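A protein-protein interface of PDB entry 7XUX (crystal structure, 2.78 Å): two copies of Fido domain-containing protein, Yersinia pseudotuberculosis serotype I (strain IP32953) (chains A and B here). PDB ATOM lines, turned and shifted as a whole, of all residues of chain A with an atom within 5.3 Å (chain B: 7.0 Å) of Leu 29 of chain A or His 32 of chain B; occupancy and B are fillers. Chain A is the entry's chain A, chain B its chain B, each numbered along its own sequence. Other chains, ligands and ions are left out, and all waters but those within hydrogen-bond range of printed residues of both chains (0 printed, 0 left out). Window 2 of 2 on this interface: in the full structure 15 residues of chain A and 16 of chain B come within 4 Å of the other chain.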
ATOM      1  N   THR A  25       2.712   8.271  24.649  1.00  0.00           N
ATOM      2  CA  THR A  25       1.287   8.072  24.403  1.00  0.00           C
ATOM      3  C   THR A  25       0.505   8.039  25.709  1.00  0.00           C
ATOM      4  O   THR A  25      -0.633   8.519  25.769  1.00  0.00           O
ATOM      5  CB  THR A  25       1.063   6.782  23.615  1.00  0.00           C
ATOM      6  OG1 THR A  25       1.458   5.660  24.414  1.00  0.00           O
ATOM      7  CG2 THR A  25       1.882   6.794  22.338  1.00  0.00           C
ATOM      8  N   GLU A  26       1.098   7.469  26.762  1.00  0.00           N
ATOM      9  CA  GLU A  26       0.457   7.458  28.073  1.00  0.00           C
ATOM     10  C   GLU A  26       0.125   8.870  28.534  1.00  0.00           C
ATOM     11  O   GLU A  26      -0.954   9.115  29.087  1.00  0.00           O
ATOM     12  CB  GLU A  26       1.363   6.762  29.086  1.00  0.00           C
ATOM     13  CG  GLU A  26       0.659   6.225  30.315  1.00  0.00           C
ATOM     14  CD  GLU A  26       1.524   6.326  31.557  1.00  0.00           C
ATOM     15  OE1 GLU A  26       2.407   7.209  31.594  1.00  0.00           O
ATOM     16  OE2 GLU A  26       1.330   5.518  32.488  1.00  0.00           O
ATOM     17  N   LEU A  27       1.041   9.815  28.312  1.00  0.00           N
ATOM     18  CA  LEU A  27       0.786  11.199  28.693  1.00  0.00           C
ATOM     19  C   LEU A  27      -0.194  11.871  27.742  1.00  0.00           C
ATOM     20  O   LEU A  27      -0.947  12.759  28.157  1.00  0.00           O
ATOM     21  CB  LEU A  27       2.101  11.974  28.747  1.00  0.00           C
ATOM     22  CG  LEU A  27       2.086  13.319  29.473  1.00  0.00           C
ATOM     23  CD1 LEU A  27       1.624  13.138  30.906  1.00  0.00           C
ATOM     24  CD2 LEU A  27       3.466  13.950  29.438  1.00  0.00           C
ATOM     25  N   GLU A  28      -0.207  11.460  26.472  1.00  0.00           N
ATOM     26  CA  GLU A  28      -1.118  12.060  25.503  1.00  0.00           C
ATOM     27  C   GLU A  28      -2.573  11.700  25.770  1.00  0.00           C
ATOM     28  O   GLU A  28      -3.469  12.394  25.278  1.00  0.00           O
ATOM     29  CB  GLU A  28      -0.722  11.644  24.085  1.00  0.00           C
ATOM     30  CG  GLU A  28       0.252  12.600  23.415  1.00  0.00           C
ATOM     31  CD  GLU A  28      -0.380  13.945  23.103  1.00  0.00           C
ATOM     32  OE1 GLU A  28      -1.515  13.965  22.588  1.00  0.00           O
ATOM     33  OE2 GLU A  28       0.255  14.984  23.369  1.00  0.00           O
ATOM     34  N   LEU A  29      -2.829  10.633  26.529  1.00  0.00           N
ATOM     35  CA  LEU A  29      -4.193  10.344  26.956  1.00  0.00           C
ATOM     36  C   LEU A  29      -4.698  11.405  27.923  1.00  0.00           C
ATOM     37  O   LEU A  29      -5.868  11.802  27.871  1.00  0.00           O
ATOM     38  CB  LEU A  29      -4.260   8.965  27.612  1.00  0.00           C
ATOM     39  CG  LEU A  29      -3.997   7.720  26.764  1.00  0.00           C
ATOM     40  CD1 LEU A  29      -4.467   6.475  27.500  1.00  0.00           C
ATOM     41  CD2 LEU A  29      -4.680   7.827  25.417  1.00  0.00           C
ATOM     42  N   LEU A  30      -3.824  11.880  28.808  1.00  0.00           N
ATOM     43  CA  LEU A  30      -4.209  12.785  29.881  1.00  0.00           C
ATOM     44  C   LEU A  30      -4.138  14.246  29.463  1.00  0.00           C
ATOM     45  O   LEU A  30      -4.863  15.079  30.019  1.00  0.00           O
ATOM     46  CB  LEU A  30      -3.320  12.546  31.109  1.00  0.00           C
ATOM     47  CG  LEU A  30      -3.471  11.276  31.964  1.00  0.00           C
ATOM     48  CD1 LEU A  30      -3.533   9.962  31.172  1.00  0.00           C
ATOM     49  CD2 LEU A  30      -2.353  11.216  32.996  1.00  0.00           C
ATOM     50  N   ARG A  31      -3.279  14.571  28.495  1.00  0.00           N
ATOM     51  CA  ARG A  31      -3.271  15.911  27.923  1.00  0.00           C
ATOM     52  C   ARG A  31      -4.562  16.200  27.164  1.00  0.00           C
ATOM     53  O   ARG A  31      -4.963  17.364  27.043  1.00  0.00           O
ATOM     54  CB  ARG A  31      -2.055  16.071  27.007  1.00  0.00           C
ATOM     55  CG  ARG A  31      -1.961  17.406  26.281  1.00  0.00           C
ATOM     56  CD  ARG A  31      -0.604  17.580  25.617  1.00  0.00           C
ATOM     57  NE  ARG A  31      -0.625  18.613  24.588  1.00  0.00           N
ATOM     58  CZ  ARG A  31       0.075  18.563  23.462  1.00  0.00           C
ATOM     59  NH1 ARG A  31       0.859  17.535  23.181  1.00  0.00           N
ATOM     60  NH2 ARG A  31      -0.014  19.570  22.598  1.00  0.00           N
ATOM     61  N   HIS A  32      -5.234  15.161  26.668  1.00  0.00           N
ATOM     62  CA  HIS A  32      -6.444  15.310  25.870  1.00  0.00           C
ATOM     63  C   HIS A  32      -7.687  14.777  26.570  1.00  0.00           C
ATOM     64  O   HIS A  32      -8.741  14.664  25.936  1.00  0.00           O
ATOM     65  CB  HIS A  32      -6.267  14.617  24.519  1.00  0.00           C
ATOM     66  CG  HIS A  32      -5.620  15.481  23.485  1.00  0.00           C
ATOM     67  ND1 HIS A  32      -4.334  15.267  23.036  1.00  0.00           N
ATOM     68  CD2 HIS A  32      -6.077  16.565  22.815  1.00  0.00           C
ATOM     69  CE1 HIS A  32      -4.027  16.181  22.134  1.00  0.00           C
ATOM     70  NE2 HIS A  32      -5.068  16.980  21.980  1.00  0.00           N
ATOM     71  N   LEU A  33      -7.592  14.440  27.853  1.00  0.00           N
ATOM     72  CA  LEU A  33      -8.754  13.996  28.612  1.00  0.00           C
ATOM     73  C   LEU A  33      -9.562  15.213  29.047  1.00  0.00           C
ATOM     74  O   LEU A  33      -9.079  16.039  29.829  1.00  0.00           O
ATOM     75  CB  LEU A  33      -8.315  13.161  29.814  1.00  0.00           C
ATOM     76  CG  LEU A  33      -9.323  12.916  30.938  1.00  0.00           C
ATOM     77  CD1 LEU A  33     -10.330  11.852  30.540  1.00  0.00           C
ATOM     78  CD2 LEU A  33      -8.597  12.508  32.210  1.00  0.00           C
ATOM     79  N   THR B  25      -1.760   6.652  17.947  1.00  0.00           N
ATOM     80  CA  THR B  25      -2.121   7.323  19.193  1.00  0.00           C
ATOM     81  C   THR B  25      -3.512   7.935  19.104  1.00  0.00           C
ATOM     82  O   THR B  25      -4.281   7.884  20.071  1.00  0.00           O
ATOM     83  CB  THR B  25      -1.094   8.403  19.534  1.00  0.00           C
ATOM     84  OG1 THR B  25      -1.297   9.540  18.685  1.00  0.00           O
ATOM     85  CG2 THR B  25       0.315   7.878  19.338  1.00  0.00           C
ATOM     86  N   LEU B  27      -6.131   6.840  17.416  1.00  0.00           N
ATOM     87  CA  LEU B  27      -7.112   5.782  17.621  1.00  0.00           C
ATOM     88  C   LEU B  27      -7.014   5.157  19.007  1.00  0.00           C
ATOM     89  O   LEU B  27      -7.971   4.515  19.452  1.00  0.00           O
ATOM     90  CB  LEU B  27      -6.955   4.715  16.536  1.00  0.00           C
ATOM     91  CG  LEU B  27      -8.135   3.770  16.308  1.00  0.00           C
ATOM     92  CD1 LEU B  27      -9.316   4.529  15.744  1.00  0.00           C
ATOM     93  CD2 LEU B  27      -7.731   2.664  15.362  1.00  0.00           C
ATOM     94  N   GLU B  28      -5.888   5.332  19.704  1.00  0.00           N
ATOM     95  CA  GLU B  28      -5.794   4.875  21.084  1.00  0.00           C
ATOM     96  C   GLU B  28      -6.503   5.810  22.054  1.00  0.00           C
ATOM     97  O   GLU B  28      -6.844   5.387  23.165  1.00  0.00           O
ATOM     98  CB  GLU B  28      -4.328   4.714  21.496  1.00  0.00           C
ATOM     99  CG  GLU B  28      -3.759   3.322  21.251  1.00  0.00           C
ATOM    100  CD  GLU B  28      -4.203   2.311  22.294  1.00  0.00           C
ATOM    101  OE1 GLU B  28      -5.336   1.797  22.183  1.00  0.00           O
ATOM    102  OE2 GLU B  28      -3.418   2.031  23.223  1.00  0.00           O
ATOM    103  N   LEU B  29      -6.727   7.068  21.662  1.00  0.00           N
ATOM    104  CA  LEU B  29      -7.535   7.968  22.478  1.00  0.00           C
ATOM    105  C   LEU B  29      -8.963   7.452  22.598  1.00  0.00           C
ATOM    106  O   LEU B  29      -9.515   7.351  23.700  1.00  0.00           O
ATOM    107  CB  LEU B  29      -7.535   9.374  21.870  1.00  0.00           C
ATOM    108  CG  LEU B  29      -6.217  10.097  21.588  1.00  0.00           C
ATOM    109  CD1 LEU B  29      -6.495  11.486  21.035  1.00  0.00           C
ATOM    110  CD2 LEU B  29      -5.364  10.190  22.837  1.00  0.00           C
ATOM    111  N   LEU B  30      -9.576   7.115  21.461  1.00  0.00           N
ATOM    112  CA  LEU B  30     -10.971   6.698  21.434  1.00  0.00           C
ATOM    113  C   LEU B  30     -11.177   5.331  22.067  1.00  0.00           C
ATOM    114  O   LEU B  30     -12.305   5.007  22.452  1.00  0.00           O
ATOM    115  CB  LEU B  30     -11.496   6.688  19.993  1.00  0.00           C
ATOM    116  CG  LEU B  30     -11.566   8.004  19.206  1.00  0.00           C
ATOM    117  CD1 LEU B  30     -10.193   8.542  18.849  1.00  0.00           C
ATOM    118  CD2 LEU B  30     -12.385   7.829  17.946  1.00  0.00           C
ATOM    119  N   ARG B  31     -10.120   4.526  22.177  1.00  0.00           N
ATOM    120  CA  ARG B  31     -10.239   3.226  22.826  1.00  0.00           C
ATOM    121  C   ARG B  31     -10.286   3.362  24.343  1.00  0.00           C
ATOM    122  O   ARG B  31     -11.048   2.653  25.010  1.00  0.00           O
ATOM    123  CB  ARG B  31      -9.076   2.326  22.411  1.00  0.00           C
ATOM    124  CG  ARG B  31      -9.244   0.871  22.807  1.00  0.00           C
ATOM    125  CD  ARG B  31      -8.471  -0.043  21.873  1.00  0.00           C
ATOM    126  NE  ARG B  31      -7.068  -0.156  22.247  1.00  0.00           N
ATOM    127  CZ  ARG B  31      -6.581  -1.091  23.050  1.00  0.00           C
ATOM    128  NH1 ARG B  31      -7.361  -2.016  23.585  1.00  0.00           N
ATOM    129  NH2 ARG B  31      -5.279  -1.101  23.322  1.00  0.00           N
ATOM    130  N   HIS B  32      -9.484   4.265  24.900  1.00  0.00           N
ATOM    131  CA  HIS B  32      -9.412   4.470  26.341  1.00  0.00           C
ATOM    132  C   HIS B  32     -10.360   5.554  26.834  1.00  0.00           C
ATOM    133  O   HIS B  32     -10.318   5.897  28.020  1.00  0.00           O
ATOM    134  CB  HIS B  32      -7.977   4.821  26.752  1.00  0.00           C
ATOM    135  CG  HIS B  32      -6.979   3.747  26.445  1.00  0.00           C
ATOM    136  ND1 HIS B  32      -6.726   3.310  25.162  1.00  0.00           N
ATOM    137  CD2 HIS B  32      -6.170   3.025  27.254  1.00  0.00           C
ATOM    138  CE1 HIS B  32      -5.806   2.363  25.195  1.00  0.00           C
ATOM    139  NE2 HIS B  32      -5.451   2.171  26.452  1.00  0.00           N
ATOM    140  N   LEU B  33     -11.203   6.100  25.959  1.00  0.00           N
ATOM    141  CA  LEU B  33     -12.143   7.142  26.352  1.00  0.00           C
ATOM    142  C   LEU B  33     -13.073   6.634  27.447  1.00  0.00           C
ATOM    143  O   LEU B  33     -13.768   5.629  27.266  1.00  0.00           O
ATOM    144  CB  LEU B  33     -12.945   7.603  25.137  1.00  0.00           C
ATOM    145  CG  LEU B  33     -14.105   8.569  25.389  1.00  0.00           C
ATOM    146  CD1 LEU B  33     -13.658  10.011  25.202  1.00  0.00           C
ATOM    147  CD2 LEU B  33     -15.276   8.244  24.476  1.00  0.00           C
ATOM    148  N   ARG B  34     -13.078   7.328  28.585  1.00  0.00           N
ATOM    149  CA  ARG B  34     -13.878   6.942  29.740  1.00  0.00           C
ATOM    150  C   ARG B  34     -15.219   7.667  29.789  1.00  0.00           C
ATOM    151  O   ARG B  34     -15.837   7.744  30.855  1.00  0.00           O
ATOM    152  CB  ARG B  34     -13.095   7.197  31.028  1.00  0.00           C
ATOM    153  CG  ARG B  34     -12.061   8.308  30.918  1.00  0.00           C
ATOM    154  CD  ARG B  34     -11.258   8.452  32.201  1.00  0.00           C
ATOM    155  NE  ARG B  34     -11.949   9.272  33.190  1.00  0.00           N
ATOM    156  CZ  ARG B  34     -11.420   9.665  34.340  1.00  0.00           C
ATOM    157  NH1 ARG B  34     -10.182   9.345  34.678  1.00  0.00           N
ATOM    158  NH2 ARG B  34     -12.151  10.400  35.173  1.00  0.00           N
ATOM    159  N   LEU B  35     -15.679   8.199  28.658  1.00  0.00           N
ATOM    160  CA  LEU B  35     -16.917   8.967  28.602  1.00  0.00           C
ATOM    161  C   LEU B  35     -18.085   8.017  28.364  1.00  0.00           C
ATOM    162  O   LEU B  35     -18.182   7.393  27.302  1.00  0.00           O
ATOM    163  CB  LEU B  35     -16.841  10.028  27.506  1.00  0.00           C
ATOM    164  CG  LEU B  35     -17.629  11.316  27.751  1.00  0.00           C
ATOM    165  CD1 LEU B  35     -17.174  11.986  29.038  1.00  0.00           C
ATOM    166  CD2 LEU B  35     -17.489  12.264  26.570  1.00  0.00           C
ATOM    167  N   PRO B 174      -0.894  -3.949  24.306  1.00  0.00           N
ATOM    168  CA  PRO B 174      -2.135  -3.373  23.757  1.00  0.00           C
ATOM    169  C   PRO B 174      -1.911  -2.227  22.783  1.00  0.00           C
ATOM    170  O   PRO B 174      -2.848  -1.862  22.062  1.00  0.00           O
ATOM    171  CB  PRO B 174      -2.899  -2.897  25.002  1.00  0.00           C
ATOM    172  CG  PRO B 174      -2.190  -3.456  26.186  1.00  0.00           C
ATOM    173  CD  PRO B 174      -0.951  -4.169  25.761  1.00  0.00           C
ATOM    174  N   LYS B 175      -0.713  -1.640  22.739  1.00  0.00           N
ATOM    175  CA  LYS B 175      -0.439  -0.623  21.729  1.00  0.00           C
ATOM    176  C   LYS B 175      -0.456  -1.218  20.326  1.00  0.00           C
ATOM    177  O   LYS B 175      -0.740  -0.509  19.354  1.00  0.00           O
ATOM    178  CB  LYS B 175       0.905   0.051  22.005  1.00  0.00           C
ATOM    179  CG  LYS B 175       2.015  -0.914  22.388  1.00  0.00           C
ATOM    180  CD  LYS B 175       3.377  -0.402  21.945  1.00  0.00           C
ATOM    181  CE  LYS B 175       4.495  -0.987  22.790  1.00  0.00           C
ATOM    182  NZ  LYS B 175       5.833  -0.499  22.355  1.00  0.00           N
ATOM    183  N   LEU B 178      -4.319  -2.304  17.477  1.00  0.00           N
ATOM    184  CA  LEU B 178      -4.944  -1.727  16.292  1.00  0.00           C
ATOM    185  C   LEU B 178      -4.110  -1.953  15.039  1.00  0.00           C
ATOM    186  O   LEU B 178      -4.672  -2.115  13.949  1.00  0.00           O
ATOM    187  CB  LEU B 178      -5.199  -0.236  16.507  1.00  0.00           C
ATOM    188  CG  LEU B 178      -6.438   0.068  17.354  1.00  0.00           C
ATOM    189  CD1 LEU B 178      -7.613  -0.783  16.884  1.00  0.00           C
ATOM    190  CD2 LEU B 178      -6.180  -0.125  18.846  1.00  0.00           C
ATOM    191  N   GLY B 214     -11.613  -3.987  22.490  1.00  0.00           N
ATOM    192  CA  GLY B 214     -12.220  -3.077  23.442  1.00  0.00           C
ATOM    193  C   GLY B 214     -12.775  -1.782  22.888  1.00  0.00           C
ATOM    194  O   GLY B 214     -12.453  -0.703  23.393  1.00  0.00           O
ATOM    195  N   PHE B 215     -13.620  -1.867  21.859  1.00  0.00           N
ATOM    196  CA  PHE B 215     -14.314  -0.697  21.342  1.00  0.00           C
ATOM    197  C   PHE B 215     -15.814  -0.722  21.600  1.00  0.00           C
ATOM    198  O   PHE B 215     -16.486   0.280  21.329  1.00  0.00           O
ATOM    199  CB  PHE B 215     -14.060  -0.543  19.835  1.00  0.00           C
ATOM    200  CG  PHE B 215     -12.671  -0.081  19.498  1.00  0.00           C
ATOM    201  CD1 PHE B 215     -11.643  -0.993  19.338  1.00  0.00           C
ATOM    202  CD2 PHE B 215     -12.393   1.268  19.351  1.00  0.00           C
ATOM    203  CE1 PHE B 215     -10.367  -0.570  19.030  1.00  0.00           C
ATOM    204  CE2 PHE B 215     -11.117   1.699  19.044  1.00  0.00           C
ATOM    205  CZ  PHE B 215     -10.102   0.780  18.884  1.00  0.00           C
ATOM    206  N   ARG B 222     -21.496   2.507  21.732  1.00  0.00           N
ATOM    207  CA  ARG B 222     -20.863   2.876  20.472  1.00  0.00           C
ATOM    208  C   ARG B 222     -21.077   1.755  19.467  1.00  0.00           C
ATOM    209  O   ARG B 222     -20.786   0.593  19.765  1.00  0.00           O
ATOM    210  CB  ARG B 222     -19.366   3.149  20.662  1.00  0.00           C
ATOM    211  CG  ARG B 222     -18.573   3.182  19.366  1.00  0.00           C
ATOM    212  CD  ARG B 222     -17.456   4.212  19.426  1.00  0.00           C
ATOM    213  NE  ARG B 222     -16.347   3.768  20.261  1.00  0.00           N
ATOM    214  CZ  ARG B 222     -15.446   4.577  20.802  1.00  0.00           C
ATOM    215  NH1 ARG B 222     -15.493   5.886  20.617  1.00  0.00           N
ATOM    216  NH2 ARG B 222     -14.474   4.059  21.547  1.00  0.00           N
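The side-chain carboxylate (OE2) of Glu 28 of chain A lies within salt-bridge range of the guanidinium group (NH1) of Arg 31 of chain A (2.6 Å). OE1 of Glu 28 of chain A is in hydrogen-bond range of ND1 of His 32 of chain A (3.1 Å). The side-chain carboxylate of Glu 28 of chain B is in salt-bridge range of the guanidinium group of Arg 31 of chain B. The backbone carbonyl oxygen (O) of Glu 28 of chain B lies within hydrogen-bond range of a ring nitrogen (ND1) of His 32 of chain B (2.9 Å).
Thr 25 of chain B touches Thr 25 of chain A. Glu 28 of chain A touches Leu 29 of chain B (O to CD2, 3.8 Å). Leu 29 of chain A touches Glu 28 of chain B. Leu 29 of chain B touches Leu 29 of chain A. CD2 of His 32 of chain B touches CD1 of Leu 29 of chain A (3.9 Å). Leu 33 of chain A touches Arg 34 of chain B (CD1 to CD, 3.9 Å).
Printed residues of chain B within 4 Å of Thr 25 of chain A: Thr 25. Printed residues of chain B within 4 Å of Leu 29 of chain A: Glu 28 (3.96 Å), Leu 29 (3.6 Å) and His 32 (3.9 Å). Leu 30 of chain A touches none of the printed residues of chain B. Of the printed residues of chain B, Leu 33 of chain A touches Arg 34. Of the printed residues of chain A, Thr 25 of chain B touches Thr 25 (3.6 Å). Leu 27 of chain B touches none of the printed residues of chain A. Printed residues of chain A within 4 Å of Leu 29 of chain B: Glu 28 (3.8 Å) and Leu 29 (3.6 Å). His 32 of chain B touches one residue of chain A. The nearest printed residue of chain A that does not touch His 32 of chain B is Leu 33 of chain A (6.5 Å). The nearest printed residue of chain A that does not touch Leu 29 of chain B is His 32 of chain A (4.7 Å).
Of the 16 printed residues of chain B, 5 touch a printed residue of chain A. Printed residues of chain B that touch a printed residue of chain A: Thr 25, Glu 28, Leu 29, His 32 and Arg 34. Hydrophobic or aromatic side chains of chain B within 4 Å of the printed part of chain A: Leu 29 and His 32. Along chain B the printed residues that touch a printed residue of chain A span positions 25 to 34. Of the 9 printed residues of chain A, 4 touch a printed residue of chain B. Printed residues of chain A that touch a printed residue of chain B: Thr 25, Glu 28, Leu 29 and Leu 33. Hydrophobic or aromatic side chains of chain A within 4 Å of the printed part of chain B: Leu 29 and Leu 33. Among the printed residues, 6 pairs touch across the chains. Among the printed residues, no Asp or Glu carboxylate lies within 4 Å of a Lys or Arg side-chain nitrogen of the other chain.
Thr 25 of chain B touches its own counterpart, Thr 25 of chain A. Glu 28 of chain A touches Leu 29 of chain B, and with the chains exchanged Leu 29 of chain A touches Glu 28 of chain B. Leu 29 of chain B touches its own counterpart, Leu 29 of chain A. Leu 29 of chain A touches His 32 of chain B, but with the chains exchanged His 32 of chain A does not touch Leu 29 of chain B (4.7 Å). Positions printed for both chains: 25, 27, 28, 29, 30, 31, 32 and 33. Of the 6 pairs that touch across the chains among the printed residues, 4 have their exchanged pair printed and touching as well.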
